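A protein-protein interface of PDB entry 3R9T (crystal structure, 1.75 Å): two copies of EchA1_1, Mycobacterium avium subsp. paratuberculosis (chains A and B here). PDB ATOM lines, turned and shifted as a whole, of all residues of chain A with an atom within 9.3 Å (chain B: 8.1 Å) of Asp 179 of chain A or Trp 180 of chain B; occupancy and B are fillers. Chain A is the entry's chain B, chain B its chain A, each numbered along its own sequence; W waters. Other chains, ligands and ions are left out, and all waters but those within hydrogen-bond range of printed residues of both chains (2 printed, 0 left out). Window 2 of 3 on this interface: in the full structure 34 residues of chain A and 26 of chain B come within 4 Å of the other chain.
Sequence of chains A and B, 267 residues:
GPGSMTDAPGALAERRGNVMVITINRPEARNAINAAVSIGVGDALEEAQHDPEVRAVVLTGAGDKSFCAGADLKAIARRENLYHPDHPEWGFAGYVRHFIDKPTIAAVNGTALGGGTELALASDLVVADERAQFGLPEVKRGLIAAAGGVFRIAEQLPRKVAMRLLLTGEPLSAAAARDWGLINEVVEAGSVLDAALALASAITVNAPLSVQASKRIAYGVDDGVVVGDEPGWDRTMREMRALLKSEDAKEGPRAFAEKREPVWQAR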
ATOM      1  N   GLN A 156     -29.188  30.549  11.457  1.00  0.00           N
ATOM      2  CA  GLN A 156     -28.165  29.509  11.446  1.00  0.00           C
ATOM      3  C   GLN A 156     -28.677  28.089  11.614  1.00  0.00           C
ATOM      4  O   GLN A 156     -27.913  27.146  11.456  1.00  0.00           O
ATOM      5  CB  GLN A 156     -27.117  29.825  12.496  1.00  0.00           C
ATOM      6  CG  GLN A 156     -26.531  31.204  12.292  1.00  0.00           C
ATOM      7  CD  GLN A 156     -25.332  31.482  13.158  1.00  0.00           C
ATOM      8  OE1 GLN A 156     -24.659  30.556  13.620  1.00  0.00           O
ATOM      9  NE2 GLN A 156     -25.052  32.763  13.397  1.00  0.00           N
ATOM     10  N   LEU A 157     -29.953  27.954  11.953  1.00  0.00           N
ATOM     11  CA  LEU A 157     -30.640  26.682  12.075  1.00  0.00           C
ATOM     12  C   LEU A 157     -31.896  26.763  11.225  1.00  0.00           C
ATOM     13  O   LEU A 157     -32.395  27.861  10.979  1.00  0.00           O
ATOM     14  CB  LEU A 157     -31.055  26.457  13.533  1.00  0.00           C
ATOM     15  CG  LEU A 157     -30.115  25.827  14.551  1.00  0.00           C
ATOM     16  CD1 LEU A 157     -30.780  25.769  15.907  1.00  0.00           C
ATOM     17  CD2 LEU A 157     -29.789  24.430  14.132  1.00  0.00           C
ATOM     18  N   PRO A 158     -32.433  25.621  10.775  1.00  0.00           N
ATOM     19  CA  PRO A 158     -33.700  25.670  10.060  1.00  0.00           C
ATOM     20  C   PRO A 158     -34.747  26.408  10.871  1.00  0.00           C
ATOM     21  O   PRO A 158     -34.828  26.282  12.088  1.00  0.00           O
ATOM     22  CB  PRO A 158     -34.074  24.202   9.911  1.00  0.00           C
ATOM     23  CG  PRO A 158     -32.770  23.512   9.870  1.00  0.00           C
ATOM     24  CD  PRO A 158     -31.928  24.241  10.870  1.00  0.00           C
ATOM     25  N   VAL A 161     -36.824  24.545  13.532  1.00  0.00           N
ATOM     26  CA  VAL A 161     -35.957  24.036  14.588  1.00  0.00           C
ATOM     27  C   VAL A 161     -35.499  25.194  15.508  1.00  0.00           C
ATOM     28  O   VAL A 161     -35.489  25.049  16.748  1.00  0.00           O
ATOM     29  CB  VAL A 161     -34.767  23.281  13.976  1.00  0.00           C
ATOM     30  CG1 VAL A 161     -33.814  22.784  15.041  1.00  0.00           C
ATOM     31  CG2 VAL A 161     -35.286  22.115  13.118  1.00  0.00           C
ATOM     32  N   LEU A 172     -30.150  21.762  23.628  1.00  0.00           N
ATOM     33  CA  LEU A 172     -29.821  21.044  22.401  1.00  0.00           C
ATOM     34  C   LEU A 172     -28.481  20.350  22.666  1.00  0.00           C
ATOM     35  O   LEU A 172     -27.556  21.001  23.162  1.00  0.00           O
ATOM     36  CB  LEU A 172     -29.679  22.078  21.263  1.00  0.00           C
ATOM     37  CG  LEU A 172     -29.531  21.593  19.821  1.00  0.00           C
ATOM     38  CD1 LEU A 172     -30.842  21.032  19.279  1.00  0.00           C
ATOM     39  CD2 LEU A 172     -29.032  22.720  18.932  1.00  0.00           C
ATOM     40  N   SER A 173     -28.365  19.045  22.390  1.00  0.00           N
ATOM     41  CA  SER A 173     -27.065  18.367  22.520  1.00  0.00           C
ATOM     42  C   SER A 173     -26.062  18.837  21.474  1.00  0.00           C
ATOM     43  O   SER A 173     -26.422  19.390  20.443  1.00  0.00           O
ATOM     44  CB  SER A 173     -27.200  16.844  22.388  1.00  0.00           C
ATOM     45  OG  SER A 173     -27.660  16.473  21.099  1.00  0.00           O
ATOM     46  N   ALA A 174     -24.794  18.567  21.728  1.00  0.00           N
ATOM     47  CA  ALA A 174     -23.749  18.873  20.752  1.00  0.00           C
ATOM     48  C   ALA A 174     -24.004  18.124  19.451  1.00  0.00           C
ATOM     49  O   ALA A 174     -23.897  18.688  18.370  1.00  0.00           O
ATOM     50  CB  ALA A 174     -22.382  18.531  21.305  1.00  0.00           C
ATOM     51  N   ALA A 175     -24.399  16.869  19.561  1.00  0.00           N
ATOM     52  CA  ALA A 175     -24.698  16.082  18.389  1.00  0.00           C
ATOM     53  C   ALA A 175     -25.844  16.682  17.565  1.00  0.00           C
ATOM     54  O   ALA A 175     -25.746  16.776  16.351  1.00  0.00           O
ATOM     55  CB  ALA A 175     -25.041  14.683  18.806  1.00  0.00           C
ATOM     56  N   ALA A 176     -26.924  17.082  18.231  1.00  0.00           N
ATOM     57  CA  ALA A 176     -28.072  17.654  17.511  1.00  0.00           C
ATOM     58  C   ALA A 176     -27.671  18.995  16.877  1.00  0.00           C
ATOM     59  O   ALA A 176     -28.069  19.302  15.745  1.00  0.00           O
ATOM     60  CB  ALA A 176     -29.280  17.840  18.442  1.00  0.00           C
ATOM     61  N   ALA A 177     -26.878  19.778  17.604  1.00  0.00           N
ATOM     62  CA  ALA A 177     -26.372  21.042  17.061  1.00  0.00           C
ATOM     63  C   ALA A 177     -25.565  20.790  15.808  1.00  0.00           C
ATOM     64  O   ALA A 177     -25.718  21.504  14.813  1.00  0.00           O
ATOM     65  CB  ALA A 177     -25.537  21.780  18.087  1.00  0.00           C
ATOM     66  N   ARG A 178     -24.726  19.760  15.831  1.00  0.00           N
ATOM     67  CA  ARG A 178     -23.930  19.425  14.664  1.00  0.00           C
ATOM     68  C   ARG A 178     -24.800  18.934  13.513  1.00  0.00           C
ATOM     69  O   ARG A 178     -24.559  19.294  12.368  1.00  0.00           O
ATOM     70  CB  ARG A 178     -22.869  18.378  15.005  1.00  0.00           C
ATOM     71  CG  ARG A 178     -21.798  18.225  13.946  1.00  0.00           C
ATOM     72  CD  ARG A 178     -21.537  16.788  13.608  1.00  0.00           C
ATOM     73  NE  ARG A 178     -22.734  16.125  13.096  1.00  0.00           N
ATOM     74  CZ  ARG A 178     -23.052  15.966  11.813  1.00  0.00           C
ATOM     75  NH1 ARG A 178     -22.273  16.423  10.835  1.00  0.00           N
ATOM     76  NH2 ARG A 178     -24.175  15.334  11.507  1.00  0.00           N
ATOM     77  N   ASP A 179     -25.811  18.126  13.811  1.00  0.00           N
ATOM     78  CA  ASP A 179     -26.683  17.586  12.770  1.00  0.00           C
ATOM     79  C   ASP A 179     -27.406  18.675  12.000  1.00  0.00           C
ATOM     80  O   ASP A 179     -27.667  18.520  10.803  1.00  0.00           O
ATOM     81  CB  ASP A 179     -27.749  16.662  13.371  1.00  0.00           C
ATOM     82  CG  ASP A 179     -27.175  15.391  13.959  1.00  0.00           C
ATOM     83  OD1 ASP A 179     -26.026  15.026  13.654  1.00  0.00           O
ATOM     84  OD2 ASP A 179     -27.898  14.739  14.749  1.00  0.00           O
ATOM     85  N   TRP A 180     -27.771  19.746  12.684  1.00  0.00           N
ATOM     86  CA  TRP A 180     -28.566  20.805  12.064  1.00  0.00           C
ATOM     87  C   TRP A 180     -27.664  21.761  11.287  1.00  0.00           C
ATOM     88  O   TRP A 180     -28.134  22.560  10.474  1.00  0.00           O
ATOM     89  CB  TRP A 180     -29.441  21.525  13.099  1.00  0.00           C
ATOM     90  CG  TRP A 180     -30.622  20.676  13.560  1.00  0.00           C
ATOM     91  CD1 TRP A 180     -30.905  20.255  14.840  1.00  0.00           C
ATOM     92  CD2 TRP A 180     -31.641  20.121  12.724  1.00  0.00           C
ATOM     93  NE1 TRP A 180     -32.043  19.484  14.840  1.00  0.00           N
ATOM     94  CE2 TRP A 180     -32.505  19.378  13.553  1.00  0.00           C
ATOM     95  CE3 TRP A 180     -31.894  20.164  11.350  1.00  0.00           C
ATOM     96  CZ2 TRP A 180     -33.608  18.700  13.052  1.00  0.00           C
ATOM     97  CZ3 TRP A 180     -32.986  19.488  10.854  1.00  0.00           C
ATOM     98  CH2 TRP A 180     -33.835  18.771  11.706  1.00  0.00           C
ATOM     99  N   GLY A 181     -26.360  21.666  11.523  1.00  0.00           N
ATOM    100  CA  GLY A 181     -25.380  22.505  10.808  1.00  0.00           C
ATOM    101  C   GLY A 181     -25.023  23.753  11.579  1.00  0.00           C
ATOM    102  O   GLY A 181     -24.351  24.670  11.096  1.00  0.00           O
ATOM    103  N   LEU A 182     -25.441  23.764  12.823  1.00  0.00           N
ATOM    104  CA  LEU A 182     -25.123  24.848  13.736  1.00  0.00           C
ATOM    105  C   LEU A 182     -23.711  24.945  14.374  1.00  0.00           C
ATOM    106  O   LEU A 182     -23.239  26.034  14.771  1.00  0.00           O
ATOM    107  CB  LEU A 182     -26.079  24.728  14.882  1.00  0.00           C
ATOM    108  CG  LEU A 182     -25.859  25.745  15.997  1.00  0.00           C
ATOM    109  CD1 LEU A 182     -26.111  27.178  15.447  1.00  0.00           C
ATOM    110  CD2 LEU A 182     -26.737  25.454  17.205  1.00  0.00           C
ATOM    111  N   ILE A 183     -23.119  23.799  14.634  1.00  0.00           N
ATOM    112  CA  ILE A 183     -21.711  23.729  14.980  1.00  0.00           C
ATOM    113  C   ILE A 183     -21.111  22.865  13.895  1.00  0.00           C
ATOM    114  O   ILE A 183     -21.841  22.185  13.146  1.00  0.00           O
ATOM    115  CB  ILE A 183     -21.457  23.177  16.391  1.00  0.00           C
ATOM    116  CG1 ILE A 183     -21.854  21.700  16.489  1.00  0.00           C
ATOM    117  CG2 ILE A 183     -22.178  24.053  17.444  1.00  0.00           C
ATOM    118  CD1 ILE A 183     -21.387  21.049  17.796  1.00  0.00           C
ATOM    119  N   ASN A 184     -19.785  22.887  13.815  1.00  0.00           N
ATOM    120  CA  ASN A 184     -19.056  22.181  12.764  1.00  0.00           C
ATOM    121  C   ASN A 184     -18.648  20.758  13.077  1.00  0.00           C
ATOM    122  O   ASN A 184     -18.656  19.900  12.171  1.00  0.00           O
ATOM    123  CB  ASN A 184     -17.825  22.983  12.395  1.00  0.00           C
ATOM    124  CG  ASN A 184     -18.182  24.319  11.779  1.00  0.00           C
ATOM    125  OD1 ASN A 184     -18.253  25.328  12.478  1.00  0.00           O
ATOM    126  ND2 ASN A 184     -18.451  24.326  10.473  1.00  0.00           N
ATOM    127  N   GLU A 185     -18.283  20.518  14.330  1.00  0.00           N
ATOM    128  CA  GLU A 185     -17.746  19.228  14.692  1.00  0.00           C
ATOM    129  C   GLU A 185     -17.849  18.945  16.190  1.00  0.00           C
ATOM    130  O   GLU A 185     -17.871  19.852  17.018  1.00  0.00           O
ATOM    131  CB  GLU A 185     -16.330  19.133  14.139  1.00  0.00           C
ATOM    132  CG  GLU A 185     -15.275  19.602  15.004  1.00  0.00           C
ATOM    133  CD  GLU A 185     -13.917  19.159  14.494  1.00  0.00           C
ATOM    134  OE1 GLU A 185     -12.966  19.881  14.775  1.00  0.00           O
ATOM    135  OE2 GLU A 185     -13.787  18.118  13.809  1.00  0.00           O
ATOM    136  N   VAL A 186     -17.985  17.658  16.493  1.00  0.00           N
ATOM    137  CA  VAL A 186     -18.102  17.155  17.839  1.00  0.00           C
ATOM    138  C   VAL A 186     -16.880  16.305  18.063  1.00  0.00           C
ATOM    139  O   VAL A 186     -16.541  15.475  17.206  1.00  0.00           O
ATOM    140  CB  VAL A 186     -19.388  16.332  18.028  1.00  0.00           C
ATOM    141  CG1 VAL A 186     -19.507  15.867  19.460  1.00  0.00           C
ATOM    142  CG2 VAL A 186     -20.620  17.194  17.686  1.00  0.00           C
ATOM    143  N   GLN B 156     -27.076  28.918   0.780  1.00  0.00           N
ATOM    144  CA  GLN B 156     -27.439  27.615   0.267  1.00  0.00           C
ATOM    145  C   GLN B 156     -26.983  26.434   1.129  1.00  0.00           C
ATOM    146  O   GLN B 156     -27.401  25.304   0.885  1.00  0.00           O
ATOM    147  CB  GLN B 156     -26.903  27.469  -1.164  1.00  0.00           C
ATOM    148  CG  GLN B 156     -27.559  28.491  -2.074  1.00  0.00           C
ATOM    149  CD  GLN B 156     -27.344  28.251  -3.547  1.00  0.00           C
ATOM    150  OE1 GLN B 156     -27.140  27.116  -3.993  1.00  0.00           O
ATOM    151  NE2 GLN B 156     -27.373  29.343  -4.326  1.00  0.00           N
ATOM    152  N   LEU B 157     -26.086  26.695   2.078  1.00  0.00           N
ATOM    153  CA  LEU B 157     -25.670  25.747   3.116  1.00  0.00           C
ATOM    154  C   LEU B 157     -25.912  26.434   4.467  1.00  0.00           C
ATOM    155  O   LEU B 157     -25.954  27.677   4.524  1.00  0.00           O
ATOM    156  CB  LEU B 157     -24.172  25.444   2.997  1.00  0.00           C
ATOM    157  CG  LEU B 157     -23.631  24.441   1.985  1.00  0.00           C
ATOM    158  CD1 LEU B 157     -22.114  24.508   1.933  1.00  0.00           C
ATOM    159  CD2 LEU B 157     -24.066  23.058   2.399  1.00  0.00           C
ATOM    160  N   PRO B 158     -26.076  25.661   5.556  1.00  0.00           N
ATOM    161  CA  PRO B 158     -26.151  26.285   6.871  1.00  0.00           C
ATOM    162  C   PRO B 158     -24.947  27.179   7.088  1.00  0.00           C
ATOM    163  O   PRO B 158     -23.879  26.800   6.655  1.00  0.00           O
ATOM    164  CB  PRO B 158     -26.085  25.089   7.819  1.00  0.00           C
ATOM    165  CG  PRO B 158     -26.689  23.961   7.032  1.00  0.00           C
ATOM    166  CD  PRO B 158     -26.159  24.189   5.647  1.00  0.00           C
ATOM    167  N   LYS B 160     -22.688  27.962   9.407  1.00  0.00           N
ATOM    168  CA  LYS B 160     -21.439  27.404   9.937  1.00  0.00           C
ATOM    169  C   LYS B 160     -20.748  26.457   8.943  1.00  0.00           C
ATOM    170  O   LYS B 160     -19.534  26.511   8.765  1.00  0.00           O
ATOM    171  CB  LYS B 160     -21.712  26.735  11.282  1.00  0.00           C
ATOM    172  CG  LYS B 160     -22.163  27.730  12.361  1.00  0.00           C
ATOM    173  CD  LYS B 160     -20.989  28.363  12.944  1.00  0.00           C
ATOM    174  CE  LYS B 160     -21.294  29.366  14.057  1.00  0.00           C
ATOM    175  NZ  LYS B 160     -21.961  30.698  13.779  1.00  0.00           N
ATOM    176  N   VAL B 161     -21.530  25.637   8.260  1.00  0.00           N
ATOM    177  CA  VAL B 161     -21.025  24.710   7.242  1.00  0.00           C
ATOM    178  C   VAL B 161     -20.455  25.471   6.034  1.00  0.00           C
ATOM    179  O   VAL B 161     -19.345  25.174   5.554  1.00  0.00           O
ATOM    180  CB  VAL B 161     -22.146  23.753   6.807  1.00  0.00           C
ATOM    181  CG1 VAL B 161     -21.651  22.768   5.727  1.00  0.00           C
ATOM    182  CG2 VAL B 161     -22.669  22.973   8.023  1.00  0.00           C
ATOM    183  N   ALA B 162     -21.197  26.484   5.583  1.00  0.00           N
ATOM    184  CA  ALA B 162     -20.714  27.390   4.564  1.00  0.00           C
ATOM    185  C   ALA B 162     -19.407  28.085   4.907  1.00  0.00           C
ATOM    186  O   ALA B 162     -18.506  28.204   4.063  1.00  0.00           O
ATOM    187  CB  ALA B 162     -21.785  28.431   4.263  1.00  0.00           C
ATOM    188  N   ARG B 164     -17.087  27.173   6.961  1.00  0.00           N
ATOM    189  CA  ARG B 164     -15.966  26.218   6.928  1.00  0.00           C
ATOM    190  C   ARG B 164     -15.472  26.035   5.490  1.00  0.00           C
ATOM    191  O   ARG B 164     -14.262  26.034   5.236  1.00  0.00           O
ATOM    192  CB  ARG B 164     -16.343  24.862   7.563  1.00  0.00           C
ATOM    193  CG  ARG B 164     -15.201  23.786   7.566  1.00  0.00           C
ATOM    194  CD  ARG B 164     -15.603  22.394   8.178  1.00  0.00           C
ATOM    195  NE  ARG B 164     -14.972  22.179   9.485  1.00  0.00           N
ATOM    196  CZ  ARG B 164     -15.168  21.158  10.332  1.00  0.00           C
ATOM    197  NH1 ARG B 164     -14.515  21.175  11.474  1.00  0.00           N
ATOM    198  NH2 ARG B 164     -15.987  20.139  10.092  1.00  0.00           N
ATOM    199  N   LEU B 165     -16.401  25.876   4.558  1.00  0.00           N
ATOM    200  CA  LEU B 165     -16.043  25.703   3.152  1.00  0.00           C
ATOM    201  C   LEU B 165     -15.299  26.917   2.621  1.00  0.00           C
ATOM    202  O   LEU B 165     -14.248  26.817   1.973  1.00  0.00           O
ATOM    203  CB  LEU B 165     -17.314  25.427   2.344  1.00  0.00           C
ATOM    204  CG  LEU B 165     -17.169  24.946   0.908  1.00  0.00           C
ATOM    205  CD1 LEU B 165     -18.355  24.056   0.537  1.00  0.00           C
ATOM    206  CD2 LEU B 165     -17.093  26.126  -0.035  1.00  0.00           C
ATOM    207  N   LEU B 172     -15.981  19.338  -0.563  1.00  0.00           N
ATOM    208  CA  LEU B 172     -17.119  18.619  -0.049  1.00  0.00           C
ATOM    209  C   LEU B 172     -17.468  17.544  -1.072  1.00  0.00           C
ATOM    210  O   LEU B 172     -17.548  17.840  -2.259  1.00  0.00           O
ATOM    211  CB  LEU B 172     -18.285  19.599   0.070  1.00  0.00           C
ATOM    212  CG  LEU B 172     -19.301  19.352   1.167  1.00  0.00           C
ATOM    213  CD1 LEU B 172     -18.638  19.291   2.535  1.00  0.00           C
ATOM    214  CD2 LEU B 172     -20.329  20.474   1.118  1.00  0.00           C
ATOM    215  N   SER B 173     -17.685  16.311  -0.627  1.00  0.00           N
ATOM    216  CA  SER B 173     -18.098  15.250  -1.538  1.00  0.00           C
ATOM    217  C   SER B 173     -19.513  15.515  -2.038  1.00  0.00           C
ATOM    218  O   SER B 173     -20.291  16.233  -1.386  1.00  0.00           O
ATOM    219  CB  SER B 173     -18.054  13.895  -0.846  1.00  0.00           C
ATOM    220  OG  SER B 173     -19.009  13.817   0.195  1.00  0.00           O
ATOM    221  N   ALA B 174     -19.850  14.913  -3.176  1.00  0.00           N
ATOM    222  CA  ALA B 174     -21.211  14.994  -3.710  1.00  0.00           C
ATOM    223  C   ALA B 174     -22.215  14.488  -2.682  1.00  0.00           C
ATOM    224  O   ALA B 174     -23.270  15.095  -2.492  1.00  0.00           O
ATOM    225  CB  ALA B 174     -21.336  14.211  -5.008  1.00  0.00           C
ATOM    226  N   ALA B 175     -21.883  13.396  -1.996  1.00  0.00           N
ATOM    227  CA  ALA B 175     -22.804  12.848  -0.999  1.00  0.00           C
ATOM    228  C   ALA B 175     -23.033  13.829   0.149  1.00  0.00           C
ATOM    229  O   ALA B 175     -24.169  14.015   0.585  1.00  0.00           O
ATOM    230  CB  ALA B 175     -22.311  11.509  -0.468  1.00  0.00           C
ATOM    231  N   ALA B 176     -21.970  14.474   0.628  1.00  0.00           N
ATOM    232  CA  ALA B 176     -22.098  15.423   1.733  1.00  0.00           C
ATOM    233  C   ALA B 176     -22.906  16.654   1.320  1.00  0.00           C
ATOM    234  O   ALA B 176     -23.708  17.152   2.115  1.00  0.00           O
ATOM    235  CB  ALA B 176     -20.715  15.830   2.280  1.00  0.00           C
ATOM    236  N   ALA B 177     -22.690  17.126   0.088  1.00  0.00           N
ATOM    237  CA  ALA B 177     -23.428  18.267  -0.465  1.00  0.00           C
ATOM    238  C   ALA B 177     -24.903  17.927  -0.529  1.00  0.00           C
ATOM    239  O   ALA B 177     -25.753  18.759  -0.222  1.00  0.00           O
ATOM    240  CB  ALA B 177     -22.924  18.632  -1.836  1.00  0.00           C
ATOM    241  N   ARG B 178     -25.206  16.697  -0.931  1.00  0.00           N
ATOM    242  CA  ARG B 178     -26.597  16.238  -1.021  1.00  0.00           C
ATOM    243  C   ARG B 178     -27.197  16.121   0.389  1.00  0.00           C
ATOM    244  O   ARG B 178     -28.329  16.562   0.646  1.00  0.00           O
ATOM    245  CB  ARG B 178     -26.654  14.917  -1.816  1.00  0.00           C
ATOM    246  CG  ARG B 178     -28.056  14.322  -2.049  1.00  0.00           C
ATOM    247  CD  ARG B 178     -28.546  13.394  -0.943  1.00  0.00           C
ATOM    248  NE  ARG B 178     -27.473  12.689  -0.236  1.00  0.00           N
ATOM    249  CZ  ARG B 178     -26.828  11.605  -0.672  1.00  0.00           C
ATOM    250  NH1 ARG B 178     -27.108  11.059  -1.850  1.00  0.00           N
ATOM    251  NH2 ARG B 178     -25.872  11.069   0.079  1.00  0.00           N
ATOM    252  N   ASP B 179     -26.431  15.585   1.332  1.00  0.00           N
ATOM    253  CA  ASP B 179     -26.925  15.489   2.709  1.00  0.00           C
ATOM    254  C   ASP B 179     -27.311  16.847   3.310  1.00  0.00           C
ATOM    255  O   ASP B 179     -28.268  16.937   4.090  1.00  0.00           O
ATOM    256  CB  ASP B 179     -25.899  14.810   3.606  1.00  0.00           C
ATOM    257  CG  ASP B 179     -25.771  13.325   3.329  1.00  0.00           C
ATOM    258  OD1 ASP B 179     -26.613  12.763   2.601  1.00  0.00           O
ATOM    259  OD2 ASP B 179     -24.808  12.725   3.846  1.00  0.00           O
ATOM    260  N   TRP B 180     -26.578  17.902   2.960  1.00  0.00           N
ATOM    261  CA  TRP B 180     -26.917  19.257   3.462  1.00  0.00           C
ATOM    262  C   TRP B 180     -28.009  19.976   2.675  1.00  0.00           C
ATOM    263  O   TRP B 180     -28.522  21.011   3.106  1.00  0.00           O
ATOM    264  CB  TRP B 180     -25.686  20.161   3.515  1.00  0.00           C
ATOM    265  CG  TRP B 180     -24.770  19.815   4.610  1.00  0.00           C
ATOM    266  CD1 TRP B 180     -23.513  19.359   4.474  1.00  0.00           C
ATOM    267  CD2 TRP B 180     -25.032  19.878   6.030  1.00  0.00           C
ATOM    268  NE1 TRP B 180     -22.960  19.116   5.707  1.00  0.00           N
ATOM    269  CE2 TRP B 180     -23.872  19.424   6.679  1.00  0.00           C
ATOM    270  CE3 TRP B 180     -26.137  20.245   6.807  1.00  0.00           C
ATOM    271  CZ2 TRP B 180     -23.768  19.351   8.064  1.00  0.00           C
ATOM    272  CZ3 TRP B 180     -26.025  20.186   8.207  1.00  0.00           C
ATOM    273  CH2 TRP B 180     -24.853  19.732   8.810  1.00  0.00           C
ATOM    274  N   GLY B 181     -28.360  19.429   1.526  1.00  0.00           N
ATOM    275  CA  GLY B 181     -29.317  20.060   0.648  1.00  0.00           C
ATOM    276  C   GLY B 181     -28.731  21.132  -0.250  1.00  0.00           C
ATOM    277  O   GLY B 181     -29.493  21.864  -0.866  1.00  0.00           O
ATOM    278  N   LEU B 182     -27.407  21.189  -0.393  1.00  0.00           N
ATOM    279  CA  LEU B 182     -26.787  22.067  -1.386  1.00  0.00           C
ATOM    280  C   LEU B 182     -27.057  21.619  -2.825  1.00  0.00           C
ATOM    281  O   LEU B 182     -27.118  22.458  -3.742  1.00  0.00           O
ATOM    282  CB  LEU B 182     -25.274  22.120  -1.158  1.00  0.00           C
ATOM    283  CG  LEU B 182     -24.414  22.968  -2.085  1.00  0.00           C
ATOM    284  CD1 LEU B 182     -24.879  24.436  -1.991  1.00  0.00           C
ATOM    285  CD2 LEU B 182     -22.941  22.802  -1.716  1.00  0.00           C
ATOM    286  N   ILE B 183     -27.124  20.299  -3.026  1.00  0.00           N
ATOM    287  CA  ILE B 183     -27.551  19.728  -4.292  1.00  0.00           C
ATOM    288  C   ILE B 183     -28.741  18.821  -4.078  1.00  0.00           C
ATOM    289  O   ILE B 183     -29.075  18.471  -2.943  1.00  0.00           O
ATOM    290  CB  ILE B 183     -26.406  18.966  -4.996  1.00  0.00           C
ATOM    291  CG1 ILE B 183     -26.014  17.688  -4.247  1.00  0.00           C
ATOM    292  CG2 ILE B 183     -25.199  19.904  -5.137  1.00  0.00           C
ATOM    293  CD1 ILE B 183     -24.972  16.833  -5.020  1.00  0.00           C
HETATM  294  O   HOH W   1     -18.714  21.889   8.931  1.00  0.00           O
HETATM  295  O   HOH W   2     -25.186  27.256  10.823  1.00  0.00           O
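The side-chain amino group (NZ) of Lys 160 of chain B lies within hydrogen-bond range of the side-chain amide oxygen (OE1) of Gln 156 of chain A.
The side-chain amide nitrogen of Asn 184 of chain A is in hydrogen-bond range of the backbone carbonyl oxygen of Lys 160 of chain B, 3.0 Å away.
The guanidinium group (NH2) of Arg 164 of chain B is in hydrogen-bond range of the backbone carbonyl oxygen (O) of Asn 184 of chain A, 3.4 Å away.
OE1 of Glu 185 of chain A is in salt-bridge range of NH1 of Arg 164 of chain B.
The backbone carbonyl oxygen (O) of Ala 177 of chain A is in hydrogen-bond range of the backbone NH (N) of Leu 182 of chain A (3.0 Å).
The side-chain carboxylate of Asp 179 of chain A lies within salt-bridge range of the guanidinium group of Arg 178 of chain A (2.9 Å).
Among the printed residues, merely in contact across the chains: Arg 178 of chain A with Trp 180 of chain B (3.6 Å), Asp 179 of chain A with Trp 180 of chain B (3.5 Å), Trp 180 of chain A with Pro 158 of chain B (3.99 Å), Trp 180 of chain A with Trp 180 of chain B (3.8 Å), Gly 181 of chain A with Pro 158 of chain B (3.7 Å), Gly 181 of chain A with Lys 160 of chain B (3.4 Å), Gly 181 of chain A with Val 161 of chain B (3.9 Å), Gly 181 of chain A with Trp 180 of chain B (3.5 Å) and Leu 182 of chain A with Lys 160 of chain B (3.1 Å).
Of the printed residues of chain A, Trp 180 of chain B touches Arg 178, Asp 179, Trp 180 and Gly 181.
No residue of chain A comes within 4 Å of Gly 181 of chain B.
Printed residues of chain B within 4 Å of Asn 184 of chain A: Lys 160 (3.0 Å) and Arg 164 (3.4 Å).
Of the printed residues of chain A, Lys 160 of chain B touches Gln 156, Gly 181, Leu 182 and Asn 184.
Ser 173 of chain A touches none of the printed residues of chain B.
The nearest residue of chain B that does not touch Asp 179 of chain A is Pro 158 of chain B (6.7 Å).
The nearest residue of chain A that does not touch Trp 180 of chain B is Leu 182 of chain A (5.7 Å).
Along chain B the printed residues that touch a printed residue of chain A span positions 158 to 180.
Of the 19 printed residues of chain A, 8 touch a printed residue of chain B.
Among the printed residues, 13 pairs touch across the chains.
Among the printed residues, Asp or Glu carboxylates within 4 Å of a Lys or Arg side-chain nitrogen of the other chain: Glu 185 of chain A with Arg 164 of chain B (3.9 Å).
Trp 180 of chain A touches Pro 158 of chain B, but with the chains exchanged Pro 158 of chain A does not touch Trp 180 of chain B (7.6 Å).
Trp 180 of chain B touches its own counterpart, Trp 180 of chain A.
Gly 181 of chain A touches Pro 158 of chain B, but with the chains exchanged Pro 158 of chain A does not touch Gly 181 of chain B (10.3 Å).
Gly 181 of chain A touches Trp 180 of chain B, but with the chains exchanged Trp 180 of chain A does not touch Gly 181 of chain B (9.5 Å).
Water W2 lies within hydrogen-bond range of the backbone carbonyl oxygen (O) of Gly 181 of chain A (2.7 Å), the backbone carbonyl oxygen (O) of Gln 156 of chain A (2.8 Å) and the backbone NH (N) of Lys 160 of chain B (3.0 Å).
Water W1 bridges ND2 of Asn 184 of chain A (2.9 Å) and NH2 of Arg 164 of chain B (3.4 Å).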
